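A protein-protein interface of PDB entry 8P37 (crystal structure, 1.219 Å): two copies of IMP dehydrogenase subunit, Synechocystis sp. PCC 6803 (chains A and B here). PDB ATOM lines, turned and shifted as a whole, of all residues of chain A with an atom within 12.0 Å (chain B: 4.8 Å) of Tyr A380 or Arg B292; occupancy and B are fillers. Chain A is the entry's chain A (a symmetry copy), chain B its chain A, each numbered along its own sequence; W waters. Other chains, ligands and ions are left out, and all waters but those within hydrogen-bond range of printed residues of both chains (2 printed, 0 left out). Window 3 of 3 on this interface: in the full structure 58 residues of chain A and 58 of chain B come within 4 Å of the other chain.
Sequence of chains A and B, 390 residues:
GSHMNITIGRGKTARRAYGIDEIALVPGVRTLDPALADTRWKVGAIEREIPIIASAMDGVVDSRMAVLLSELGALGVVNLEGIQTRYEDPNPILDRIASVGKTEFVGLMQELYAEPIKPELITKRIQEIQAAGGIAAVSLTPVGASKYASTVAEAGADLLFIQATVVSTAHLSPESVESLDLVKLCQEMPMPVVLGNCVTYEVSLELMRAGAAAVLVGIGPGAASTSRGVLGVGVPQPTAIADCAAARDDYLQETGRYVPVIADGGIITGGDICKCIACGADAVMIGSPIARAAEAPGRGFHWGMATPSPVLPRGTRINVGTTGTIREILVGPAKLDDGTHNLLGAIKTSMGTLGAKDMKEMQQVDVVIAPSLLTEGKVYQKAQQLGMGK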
ATOM      1  N   ASP A 337       7.894 -15.069  -5.609  1.00  0.00           N
ATOM      2  CA  ASP A 337       8.402 -13.754  -5.956  1.00  0.00           C
ATOM      3  C   ASP A 337       9.070 -13.656  -7.277  1.00  0.00           C
ATOM      4  O   ASP A 337       9.691 -12.635  -7.517  1.00  0.00           O
ATOM      5  CB  ASP A 337       9.377 -13.370  -4.887  1.00  0.00           C
ATOM      6  CG  ASP A 337      10.590 -14.264  -4.740  1.00  0.00           C
ATOM      7  OD1 ASP A 337      10.885 -15.064  -5.664  1.00  0.00           O
ATOM      8  OD2 ASP A 337      11.245 -14.209  -3.679  1.00  0.00           O
ATOM      9  N   LEU A 374      18.578  -8.505 -16.830  1.00  0.00           N
ATOM     10  CA  LEU A 374      18.462  -9.556 -15.815  1.00  0.00           C
ATOM     11  C   LEU A 374      19.624  -9.671 -14.878  1.00  0.00           C
ATOM     12  O   LEU A 374      19.556 -10.511 -13.964  1.00  0.00           O
ATOM     13  CB  LEU A 374      18.166 -10.895 -16.479  1.00  0.00           C
ATOM     14  CG  LEU A 374      16.957 -10.954 -17.469  1.00  0.00           C
ATOM     15  CD1 LEU A 374      16.963 -12.277 -18.203  1.00  0.00           C
ATOM     16  CD2 LEU A 374      15.667 -10.734 -16.794  1.00  0.00           C
ATOM     17  N   THR A 375      20.662  -8.851 -15.019  1.00  0.00           N
ATOM     18  CA  THR A 375      21.827  -8.933 -14.155  1.00  0.00           C
ATOM     19  C   THR A 375      22.081  -7.658 -13.319  1.00  0.00           C
ATOM     20  O   THR A 375      22.616  -7.753 -12.223  1.00  0.00           O
ATOM     21  CB  THR A 375      23.052  -9.262 -15.010  1.00  0.00           C
ATOM     22  OG1 THR A 375      23.230  -8.187 -15.922  1.00  0.00           O
ATOM     23  CG2 THR A 375      22.889 -10.584 -15.775  1.00  0.00           C
ATOM     24  N   GLU A 376      21.701  -6.473 -13.801  1.00  0.00           N
ATOM     25  CA  GLU A 376      21.941  -5.208 -13.096  1.00  0.00           C
ATOM     26  C   GLU A 376      21.356  -5.246 -11.685  1.00  0.00           C
ATOM     27  O   GLU A 376      20.176  -5.498 -11.531  1.00  0.00           O
ATOM     28  CB  GLU A 376      21.328  -4.063 -13.926  1.00  0.00           C
ATOM     29  CG  GLU A 376      21.541  -2.661 -13.413  1.00  0.00           C
ATOM     30  CD  GLU A 376      21.019  -1.652 -14.431  1.00  0.00           C
ATOM     31  OE1 GLU A 376      19.797  -1.674 -14.694  1.00  0.00           O
ATOM     32  OE2 GLU A 376      21.803  -0.805 -14.926  1.00  0.00           O
ATOM     33  N   GLY A 377      22.182  -5.080 -10.670  1.00  0.00           N
ATOM     34  CA  GLY A 377      21.769  -5.133  -9.280  1.00  0.00           C
ATOM     35  C   GLY A 377      21.490  -6.494  -8.681  1.00  0.00           C
ATOM     36  O   GLY A 377      21.223  -6.567  -7.479  1.00  0.00           O
ATOM     37  N   LYS A 378      21.621  -7.586  -9.450  1.00  0.00           N
ATOM     38  CA  LYS A 378      21.111  -8.887  -9.033  1.00  0.00           C
ATOM     39  C   LYS A 378      22.127  -9.805  -8.388  1.00  0.00           C
ATOM     40  O   LYS A 378      21.825 -10.984  -8.213  1.00  0.00           O
ATOM     41  CB  LYS A 378      20.440  -9.558 -10.238  1.00  0.00           C
ATOM     42  CG  LYS A 378      19.329  -8.696 -10.849  1.00  0.00           C
ATOM     43  CD  LYS A 378      18.155  -8.374  -9.876  1.00  0.00           C
ATOM     44  CE  LYS A 378      17.171  -7.362 -10.439  1.00  0.00           C
ATOM     45  NZ  LYS A 378      17.640  -5.948 -10.308  1.00  0.00           N
ATOM     46  N   VAL A 379      23.284  -9.308  -7.959  1.00  0.00           N
ATOM     47  CA  VAL A 379      24.316 -10.184  -7.394  1.00  0.00           C
ATOM     48  C   VAL A 379      23.829 -10.985  -6.181  1.00  0.00           C
ATOM     49  O   VAL A 379      24.177 -12.157  -6.059  1.00  0.00           O
ATOM     50  CB  VAL A 379      25.610  -9.393  -7.075  1.00  0.00           C
ATOM     51  CG1 VAL A 379      25.379  -8.345  -6.019  1.00  0.00           C
ATOM     52  CG2 VAL A 379      26.748 -10.327  -6.653  1.00  0.00           C
ATOM     53  N   TYR A 380      23.063 -10.375  -5.276  1.00  0.00           N
ATOM     54  CA  TYR A 380      22.610 -11.110  -4.092  1.00  0.00           C
ATOM     55  C   TYR A 380      21.593 -12.170  -4.483  1.00  0.00           C
ATOM     56  O   TYR A 380      21.595 -13.264  -3.914  1.00  0.00           O
ATOM     57  CB  TYR A 380      21.958 -10.146  -3.085  1.00  0.00           C
ATOM     58  CG  TYR A 380      22.887  -9.138  -2.447  1.00  0.00           C
ATOM     59  CD1 TYR A 380      23.645  -9.476  -1.340  1.00  0.00           C
ATOM     60  CD2 TYR A 380      22.931  -7.819  -2.885  1.00  0.00           C
ATOM     61  CE1 TYR A 380      24.448  -8.544  -0.705  1.00  0.00           C
ATOM     62  CE2 TYR A 380      23.686  -6.865  -2.212  1.00  0.00           C
ATOM     63  CZ  TYR A 380      24.454  -7.240  -1.136  1.00  0.00           C
ATOM     64  OH  TYR A 380      25.212  -6.337  -0.422  1.00  0.00           O
ATOM     65  N   GLN A 381      20.694 -11.852  -5.381  1.00  0.00           N
ATOM     66  CA  GLN A 381      19.670 -12.799  -5.828  1.00  0.00           C
ATOM     67  C   GLN A 381      20.314 -14.017  -6.501  1.00  0.00           C
ATOM     68  O   GLN A 381      19.916 -15.157  -6.232  1.00  0.00           O
ATOM     69  CB  GLN A 381      18.654 -12.148  -6.767  1.00  0.00           C
ATOM     70  CG  GLN A 381      17.727 -11.165  -6.054  1.00  0.00           C
ATOM     71  CD  GLN A 381      16.722 -10.567  -6.982  1.00  0.00           C
ATOM     72  OE1 GLN A 381      16.143 -11.243  -7.864  1.00  0.00           O
ATOM     73  NE2 GLN A 381      16.456  -9.288  -6.802  1.00  0.00           N
ATOM     74  N   LYS A 382      21.354 -13.783  -7.281  1.00  0.00           N
ATOM     75  CA  LYS A 382      22.090 -14.877  -7.915  1.00  0.00           C
ATOM     76  C   LYS A 382      22.829 -15.692  -6.852  1.00  0.00           C
ATOM     77  O   LYS A 382      22.762 -16.928  -6.887  1.00  0.00           O
ATOM     78  CB  LYS A 382      23.085 -14.313  -8.934  1.00  0.00           C
ATOM     79  N   ALA A 383      23.523 -15.048  -5.917  1.00  0.00           N
ATOM     80  CA  ALA A 383      24.301 -15.756  -4.915  1.00  0.00           C
ATOM     81  C   ALA A 383      23.435 -16.572  -4.016  1.00  0.00           C
ATOM     82  O   ALA A 383      23.839 -17.652  -3.591  1.00  0.00           O
ATOM     83  CB  ALA A 383      25.108 -14.763  -4.076  1.00  0.00           C
ATOM     84  N   GLN A 384      22.258 -16.059  -3.654  1.00  0.00           N
ATOM     85  CA  GLN A 384      21.393 -16.691  -2.652  1.00  0.00           C
ATOM     86  C   GLN A 384      20.267 -17.512  -3.245  1.00  0.00           C
ATOM     87  O   GLN A 384      19.484 -18.083  -2.491  1.00  0.00           O
ATOM     88  CB  GLN A 384      20.838 -15.608  -1.697  1.00  0.00           C
ATOM     89  CG  GLN A 384      21.949 -14.917  -0.921  1.00  0.00           C
ATOM     90  CD  GLN A 384      21.538 -13.694  -0.154  1.00  0.00           C
ATOM     91  OE1 GLN A 384      20.411 -13.563   0.307  1.00  0.00           O
ATOM     92  NE2 GLN A 384      22.478 -12.779   0.040  1.00  0.00           N
ATOM     93  N   GLN A 385      20.184 -17.579  -4.573  1.00  0.00           N
ATOM     94  CA  GLN A 385      19.178 -18.351  -5.297  1.00  0.00           C
ATOM     95  C   GLN A 385      17.779 -17.936  -4.865  1.00  0.00           C
ATOM     96  O   GLN A 385      16.956 -18.767  -4.426  1.00  0.00           O
ATOM     97  CB  GLN A 385      19.423 -19.863  -5.095  1.00  0.00           C
ATOM     98  CG  GLN A 385      20.776 -20.304  -5.628  1.00  0.00           C
ATOM     99  CD  GLN A 385      20.878 -21.807  -5.653  1.00  0.00           C
ATOM    100  OE1 GLN A 385      20.494 -22.457  -6.626  1.00  0.00           O
ATOM    101  NE2 GLN A 385      21.386 -22.400  -4.582  1.00  0.00           N
ATOM    102  N   LEU A 386      17.543 -16.636  -4.975  1.00  0.00           N
ATOM    103  CA  LEU A 386      16.290 -16.011  -4.604  1.00  0.00           C
ATOM    104  C   LEU A 386      15.810 -15.147  -5.716  1.00  0.00           C
ATOM    105  O   LEU A 386      16.616 -14.697  -6.524  1.00  0.00           O
ATOM    106  CB  LEU A 386      16.490 -15.119  -3.338  1.00  0.00           C
ATOM    107  CG  LEU A 386      16.792 -15.851  -2.024  1.00  0.00           C
ATOM    108  CD1 LEU A 386      17.306 -14.903  -0.974  1.00  0.00           C
ATOM    109  CD2 LEU A 386      15.590 -16.619  -1.518  1.00  0.00           C
ATOM    110  N   GLY A 387      14.507 -14.885  -5.769  1.00  0.00           N
ATOM    111  CA  GLY A 387      13.957 -13.971  -6.759  1.00  0.00           C
ATOM    112  C   GLY A 387      14.222 -14.393  -8.196  1.00  0.00           C
ATOM    113  O   GLY A 387      13.834 -15.501  -8.598  1.00  0.00           O
ATOM    114  N   MET A 388      14.884 -13.528  -8.972  1.00  0.00           N
ATOM    115  CA  MET A 388      15.274 -13.771 -10.350  1.00  0.00           C
ATOM    116  C   MET A 388      16.468 -14.753 -10.448  1.00  0.00           C
ATOM    117  O   MET A 388      16.754 -15.229 -11.549  1.00  0.00           O
ATOM    118  CB  MET A 388      15.598 -12.439 -11.059  1.00  0.00           C
ATOM    119  CG  MET A 388      14.368 -11.487 -11.194  1.00  0.00           C
ATOM    120  SD  MET A 388      14.760  -9.805 -11.815  1.00  0.00           S
ATOM    121  CE  MET A 388      15.393 -10.197 -13.429  1.00  0.00           C
ATOM    122  N   GLY A 389      17.114 -15.106  -9.331  1.00  0.00           N
ATOM    123  CA  GLY A 389      18.269 -15.999  -9.347  1.00  0.00           C
ATOM    124  C   GLY A 389      18.070 -17.394  -8.800  1.00  0.00           C
ATOM    125  O   GLY A 389      19.071 -18.114  -8.609  1.00  0.00           O
ATOM    126  N   ALA B 223      18.447  -4.361  -5.915  1.00  0.00           N
ATOM    127  CA  ALA B 223      18.963  -5.615  -5.403  1.00  0.00           C
ATOM    128  C   ALA B 223      17.865  -6.554  -4.888  1.00  0.00           C
ATOM    129  O   ALA B 223      18.054  -7.785  -4.880  1.00  0.00           O
ATOM    130  CB  ALA B 223      19.970  -5.352  -4.305  1.00  0.00           C
ATOM    131  N   ILE B 268      25.585  -0.769  -5.404  1.00  0.00           N
ATOM    132  CA  ILE B 268      26.174  -1.496  -4.287  1.00  0.00           C
ATOM    133  C   ILE B 268      27.425  -0.746  -3.765  1.00  0.00           C
ATOM    134  O   ILE B 268      27.668  -0.721  -2.575  1.00  0.00           O
ATOM    135  CB  ILE B 268      26.517  -2.950  -4.749  1.00  0.00           C
ATOM    136  CG1 ILE B 268      25.170  -3.687  -4.985  1.00  0.00           C
ATOM    137  CG2 ILE B 268      27.384  -3.696  -3.712  1.00  0.00           C
ATOM    138  CD1 ILE B 268      25.249  -4.957  -5.646  1.00  0.00           C
ATOM    139  N   SER B 288      20.016  -1.132  -0.511  1.00  0.00           N
ATOM    140  CA  SER B 288      20.814  -2.235   0.013  1.00  0.00           C
ATOM    141  C   SER B 288      22.100  -1.790   0.724  1.00  0.00           C
ATOM    142  O   SER B 288      22.423  -2.414   1.754  1.00  0.00           O
ATOM    143  CB  SER B 288      21.110  -3.279  -1.065  1.00  0.00           C
ATOM    144  OG  SER B 288      22.237  -2.942  -1.868  1.00  0.00           O
ATOM    145  N   PRO B 289      22.824  -0.778   0.264  1.00  0.00           N
ATOM    146  CA  PRO B 289      24.060  -0.421   0.983  1.00  0.00           C
ATOM    147  C   PRO B 289      23.813   0.095   2.394  1.00  0.00           C
ATOM    148  O   PRO B 289      24.689   0.029   3.251  1.00  0.00           O
ATOM    149  CB  PRO B 289      24.689   0.657   0.111  1.00  0.00           C
ATOM    150  CG  PRO B 289      24.141   0.380  -1.227  1.00  0.00           C
ATOM    151  CD  PRO B 289      22.722   0.013  -0.989  1.00  0.00           C
ATOM    152  N   ILE B 290      22.626   0.674   2.611  1.00  0.00           N
ATOM    153  CA  ILE B 290      22.234   1.259   3.902  1.00  0.00           C
ATOM    154  C   ILE B 290      21.576   0.215   4.800  1.00  0.00           C
ATOM    155  O   ILE B 290      21.742   0.243   6.028  1.00  0.00           O
ATOM    156  CB  ILE B 290      21.363   2.532   3.629  1.00  0.00           C
ATOM    157  CG1 ILE B 290      22.297   3.619   2.997  1.00  0.00           C
ATOM    158  CG2 ILE B 290      20.777   3.069   4.925  1.00  0.00           C
ATOM    159  CD1 ILE B 290      21.681   4.907   2.543  1.00  0.00           C
ATOM    160  N   ALA B 291      20.909  -0.772   4.180  1.00  0.00           N
ATOM    161  CA  ALA B 291      20.391  -1.927   4.934  1.00  0.00           C
ATOM    162  C   ALA B 291      21.535  -2.702   5.588  1.00  0.00           C
ATOM    163  O   ALA B 291      21.294  -3.479   6.505  1.00  0.00           O
ATOM    164  CB  ALA B 291      19.580  -2.825   4.016  1.00  0.00           C
ATOM    165  N   ARG B 292      22.793  -2.506   5.179  1.00  0.00           N
ATOM    166  CA  ARG B 292      23.953  -3.150   5.791  1.00  0.00           C
ATOM    167  C   ARG B 292      24.456  -2.437   7.058  1.00  0.00           C
ATOM    168  O   ARG B 292      25.426  -2.883   7.686  1.00  0.00           O
ATOM    169  CB  ARG B 292      25.075  -3.253   4.762  1.00  0.00           C
ATOM    170  CG  ARG B 292      24.730  -4.110   3.589  1.00  0.00           C
ATOM    171  CD  ARG B 292      25.859  -4.269   2.608  1.00  0.00           C
ATOM    172  NE  ARG B 292      26.444  -5.589   2.681  1.00  0.00           N
ATOM    173  CZ  ARG B 292      27.529  -5.978   2.020  1.00  0.00           C
ATOM    174  NH1 ARG B 292      28.155  -5.138   1.201  1.00  0.00           N
ATOM    175  NH2 ARG B 292      27.978  -7.219   2.148  1.00  0.00           N
ATOM    176  N   ALA B 293      23.801  -1.348   7.460  1.00  0.00           N
ATOM    177  CA  ALA B 293      24.198  -0.597   8.635  1.00  0.00           C
ATOM    178  C   ALA B 293      23.779  -1.294   9.889  1.00  0.00           C
ATOM    179  O   ALA B 293      22.702  -1.905   9.955  1.00  0.00           O
ATOM    180  CB  ALA B 293      23.643   0.811   8.631  1.00  0.00           C
ATOM    181  N   ALA B 294      24.545  -1.107  10.948  1.00  0.00           N
ATOM    182  CA  ALA B 294      24.204  -1.643  12.263  1.00  0.00           C
ATOM    183  C   ALA B 294      22.845  -1.135  12.722  1.00  0.00           C
ATOM    184  O   ALA B 294      22.132  -1.860  13.417  1.00  0.00           O
ATOM    185  CB  ALA B 294      25.256  -1.264  13.288  1.00  0.00           C
ATOM    186  N   ALA B 296      20.241  -0.344  10.791  1.00  0.00           N
ATOM    187  CA  ALA B 296      19.189  -0.604   9.806  1.00  0.00           C
ATOM    188  C   ALA B 296      18.084  -1.443  10.390  1.00  0.00           C
ATOM    189  O   ALA B 296      18.313  -2.449  11.113  1.00  0.00           O
ATOM    190  CB  ALA B 296      19.745  -1.244   8.556  1.00  0.00           C
ATOM    191  N   ILE B 318      16.421 -10.435   0.517  1.00  0.00           N
ATOM    192  CA  ILE B 318      17.811 -10.894   0.457  1.00  0.00           C
ATOM    193  C   ILE B 318      18.493 -10.646   1.813  1.00  0.00           C
ATOM    194  O   ILE B 318      18.066  -9.809   2.622  1.00  0.00           O
ATOM    195  CB  ILE B 318      18.615 -10.244  -0.705  1.00  0.00           C
ATOM    196  CG1 ILE B 318      18.577  -8.720  -0.602  1.00  0.00           C
ATOM    197  CG2 ILE B 318      18.119 -10.725  -2.038  1.00  0.00           C
ATOM    198  CD1 ILE B 318      19.516  -7.959  -1.456  1.00  0.00           C
ATOM    199  N   ASN B 319      19.580 -11.383   2.043  1.00  0.00           N
ATOM    200  CA  ASN B 319      20.389 -11.246   3.227  1.00  0.00           C
ATOM    201  C   ASN B 319      21.602 -10.408   2.851  1.00  0.00           C
ATOM    202  O   ASN B 319      22.459 -10.867   2.086  1.00  0.00           O
ATOM    203  CB  ASN B 319      20.790 -12.627   3.718  1.00  0.00           C
ATOM    204  CG  ASN B 319      21.515 -12.666   5.035  1.00  0.00           C
ATOM    205  OD1 ASN B 319      21.881 -11.653   5.607  1.00  0.00           O
ATOM    206  ND2 ASN B 319      21.667 -13.840   5.596  1.00  0.00           N
ATOM    207  N   VAL B 320      21.640  -9.141   3.274  1.00  0.00           N
ATOM    208  CA  VAL B 320      22.772  -8.273   2.977  1.00  0.00           C
ATOM    209  C   VAL B 320      23.841  -8.256   4.077  1.00  0.00           C
ATOM    210  O   VAL B 320      25.019  -7.860   3.832  1.00  0.00           O
ATOM    211  CB  VAL B 320      22.316  -6.831   2.620  1.00  0.00           C
ATOM    212  CG1 VAL B 320      21.419  -6.817   1.386  1.00  0.00           C
ATOM    213  CG2 VAL B 320      21.624  -6.152   3.796  1.00  0.00           C
ATOM    214  N   GLY B 321      23.497  -8.743   5.253  1.00  0.00           N
ATOM    215  CA  GLY B 321      24.385  -8.717   6.380  1.00  0.00           C
ATOM    216  C   GLY B 321      24.526  -7.336   6.985  1.00  0.00           C
ATOM    217  O   GLY B 321      23.792  -6.389   6.634  1.00  0.00           O
ATOM    218  N   THR B 322      25.444  -7.222   7.945  1.00  0.00           N
ATOM    219  CA  THR B 322      25.682  -5.974   8.679  1.00  0.00           C
ATOM    220  C   THR B 322      27.165  -5.786   8.675  1.00  0.00           C
ATOM    221  O   THR B 322      27.897  -6.619   9.230  1.00  0.00           O
ATOM    222  CB  THR B 322      25.129  -6.081  10.079  1.00  0.00           C
ATOM    223  OG1 THR B 322      23.708  -6.377  10.002  1.00  0.00           O
ATOM    224  CG2 THR B 322      25.341  -4.818  10.868  1.00  0.00           C
ATOM    225  N   THR B 323      27.643  -4.689   8.074  1.00  0.00           N
ATOM    226  CA  THR B 323      29.083  -4.485   7.893  1.00  0.00           C
ATOM    227  C   THR B 323      29.718  -3.303   8.587  1.00  0.00           C
ATOM    228  O   THR B 323      30.959  -3.211   8.625  1.00  0.00           O
ATOM    229  CB  THR B 323      29.386  -4.364   6.422  1.00  0.00           C
ATOM    230  OG1 THR B 323      28.871  -3.121   5.924  1.00  0.00           O
ATOM    231  CG2 THR B 323      28.826  -5.508   5.599  1.00  0.00           C
ATOM    232  N   GLY B 324      28.913  -2.437   9.185  1.00  0.00           N
ATOM    233  CA  GLY B 324      29.419  -1.250   9.852  1.00  0.00           C
ATOM    234  C   GLY B 324      28.277  -0.374  10.287  1.00  0.00           C
ATOM    235  O   GLY B 324      27.103  -0.696  10.043  1.00  0.00           O
ATOM    236  N   ILE B 329      29.497   3.569   6.741  1.00  0.00           N
ATOM    237  CA  ILE B 329      29.036   3.335   5.380  1.00  0.00           C
ATOM    238  C   ILE B 329      29.026   4.619   4.579  1.00  0.00           C
ATOM    239  O   ILE B 329      29.478   4.623   3.433  1.00  0.00           O
ATOM    240  CB  ILE B 329      27.636   2.634   5.374  1.00  0.00           C
ATOM    241  CG1 ILE B 329      27.823   1.161   5.830  1.00  0.00           C
ATOM    242  CG2 ILE B 329      26.988   2.740   3.984  1.00  0.00           C
ATOM    243  CD1 ILE B 329      26.589   0.504   6.302  1.00  0.00           C
ATOM    244  N   THR B 340      32.130  -0.460  -0.487  1.00  0.00           N
ATOM    245  CA  THR B 340      30.785  -0.399   0.094  1.00  0.00           C
ATOM    246  C   THR B 340      30.732   0.405   1.382  1.00  0.00           C
ATOM    247  O   THR B 340      29.614   0.632   1.898  1.00  0.00           O
ATOM    248  CB  THR B 340      30.200  -1.788   0.267  1.00  0.00           C
ATOM    249  OG1 THR B 340      30.912  -2.451   1.330  1.00  0.00           O
ATOM    250  CG2 THR B 340      30.151  -2.571  -1.021  1.00  0.00           C
HETATM  251  O   HOH W   1      20.581  -8.693  -5.777  1.00  0.00           O
HETATM  252  O   HOH W   2      24.708  -3.799  -1.004  1.00  0.00           O
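O of Asn B319 sits at hydrogen-bond distance from NE2 of Gln A384 (2.8 Å).
NE of Arg B292 lies close to OH of Tyr A380 (3.4 Å).
The backbone carbonyl oxygen (O) of Ala B223 is in hydrogen-bond range of the side-chain amide nitrogen (NE2) of Gln A381 (2.9 Å).
The backbone NH of Thr B323 sits at hydrogen-bond distance from the backbone carbonyl oxygen of Arg B292 (2.9 Å).
The side-chain amide oxygen (OD1) of Asn B319 sits at hydrogen-bond distance from the backbone NH (N) of Gly B321, 3.3 Å away.
O of Gln A381 is in hydrogen-bond range of N of Leu A386, 3.1 Å away.
O of Val B320 is in hydrogen-bond range of NE of Arg B292.
The side-chain amide oxygen (OE1) of Gln A381 is in hydrogen-bond range of the backbone NH (N) of Met A388 (2.8 Å).
Among the printed residues, merely in contact across the chains: Gly A377 with Ala B223, Val A379 with Ile B268, Tyr A380 with Ile B318, Tyr A380 with Asn B319, Tyr A380 with Val B320 and Gln A384 with Ile B318.
Tyr A380 touches four residues of chain B.
Printed residues of chain A within 4 Å of Arg B292: Tyr A380 (3.4 Å).
No residue of chain A comes within 4 Å of Ser B288.
Pro B289 touches none of the printed residues of chain A.
Ile B290 touches none of the printed residues of chain A.
Ala B291 touches none of the printed residues of chain A.
No residue of chain A comes within 4 Å of Ala B296.
Of chain A, only Tyr A380 and Gln A384 come within 4 Å of Ile B318.
No residue of chain A comes within 4 Å of Thr B322.
No residue of chain A comes within 4 Å of Gly B324.
No residue of chain A comes within 4 Å of Thr B340.
Printed residues of chain B within 4 Å of Val A379: Ile B268.
Of the printed residues of chain A, Asn B319 touches Tyr A380 and Gln A384.
Of the printed residues of chain B, Gln A384 touches Ile B318 (3.7 Å) and Asn B319 (2.8 Å).
Of the printed residues of chain B, Gly A377 touches Ala B223 (3.2 Å).
Lys A382 touches none of the printed residues of chain B.
Gly A387 touches none of the printed residues of chain B.
The nearest residue of chain A that does not touch Arg B292 is Gln A384 (8.1 Å).
Of the 17 printed residues of chain A, 5 touch a printed residue of chain B.
Printed residues of chain B that touch a printed residue of chain A: Ala B223, Ile B268, Arg B292, Ile B318, Asn B319 and Val B320.
No position is printed for both chains.
Of the 9 pairs that touch across the chains among the printed residues, none has its exchanged pair printed and touching as well.
Water W2 lies within hydrogen-bond range of the side-chain hydroxyl of Tyr A380 (2.7 Å) and the side-chain hydroxyl of Ser B288 (2.8 Å).
Water W1 lies within hydrogen-bond range of the backbone carbonyl oxygen (O) of Gly A377 (2.8 Å), the backbone carbonyl oxygen (O) of Ala B223 (2.8 Å), the backbone NH (N) of Tyr A380 (3.0 Å) and the backbone NH (N) of Gln A381 (3.2 Å).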
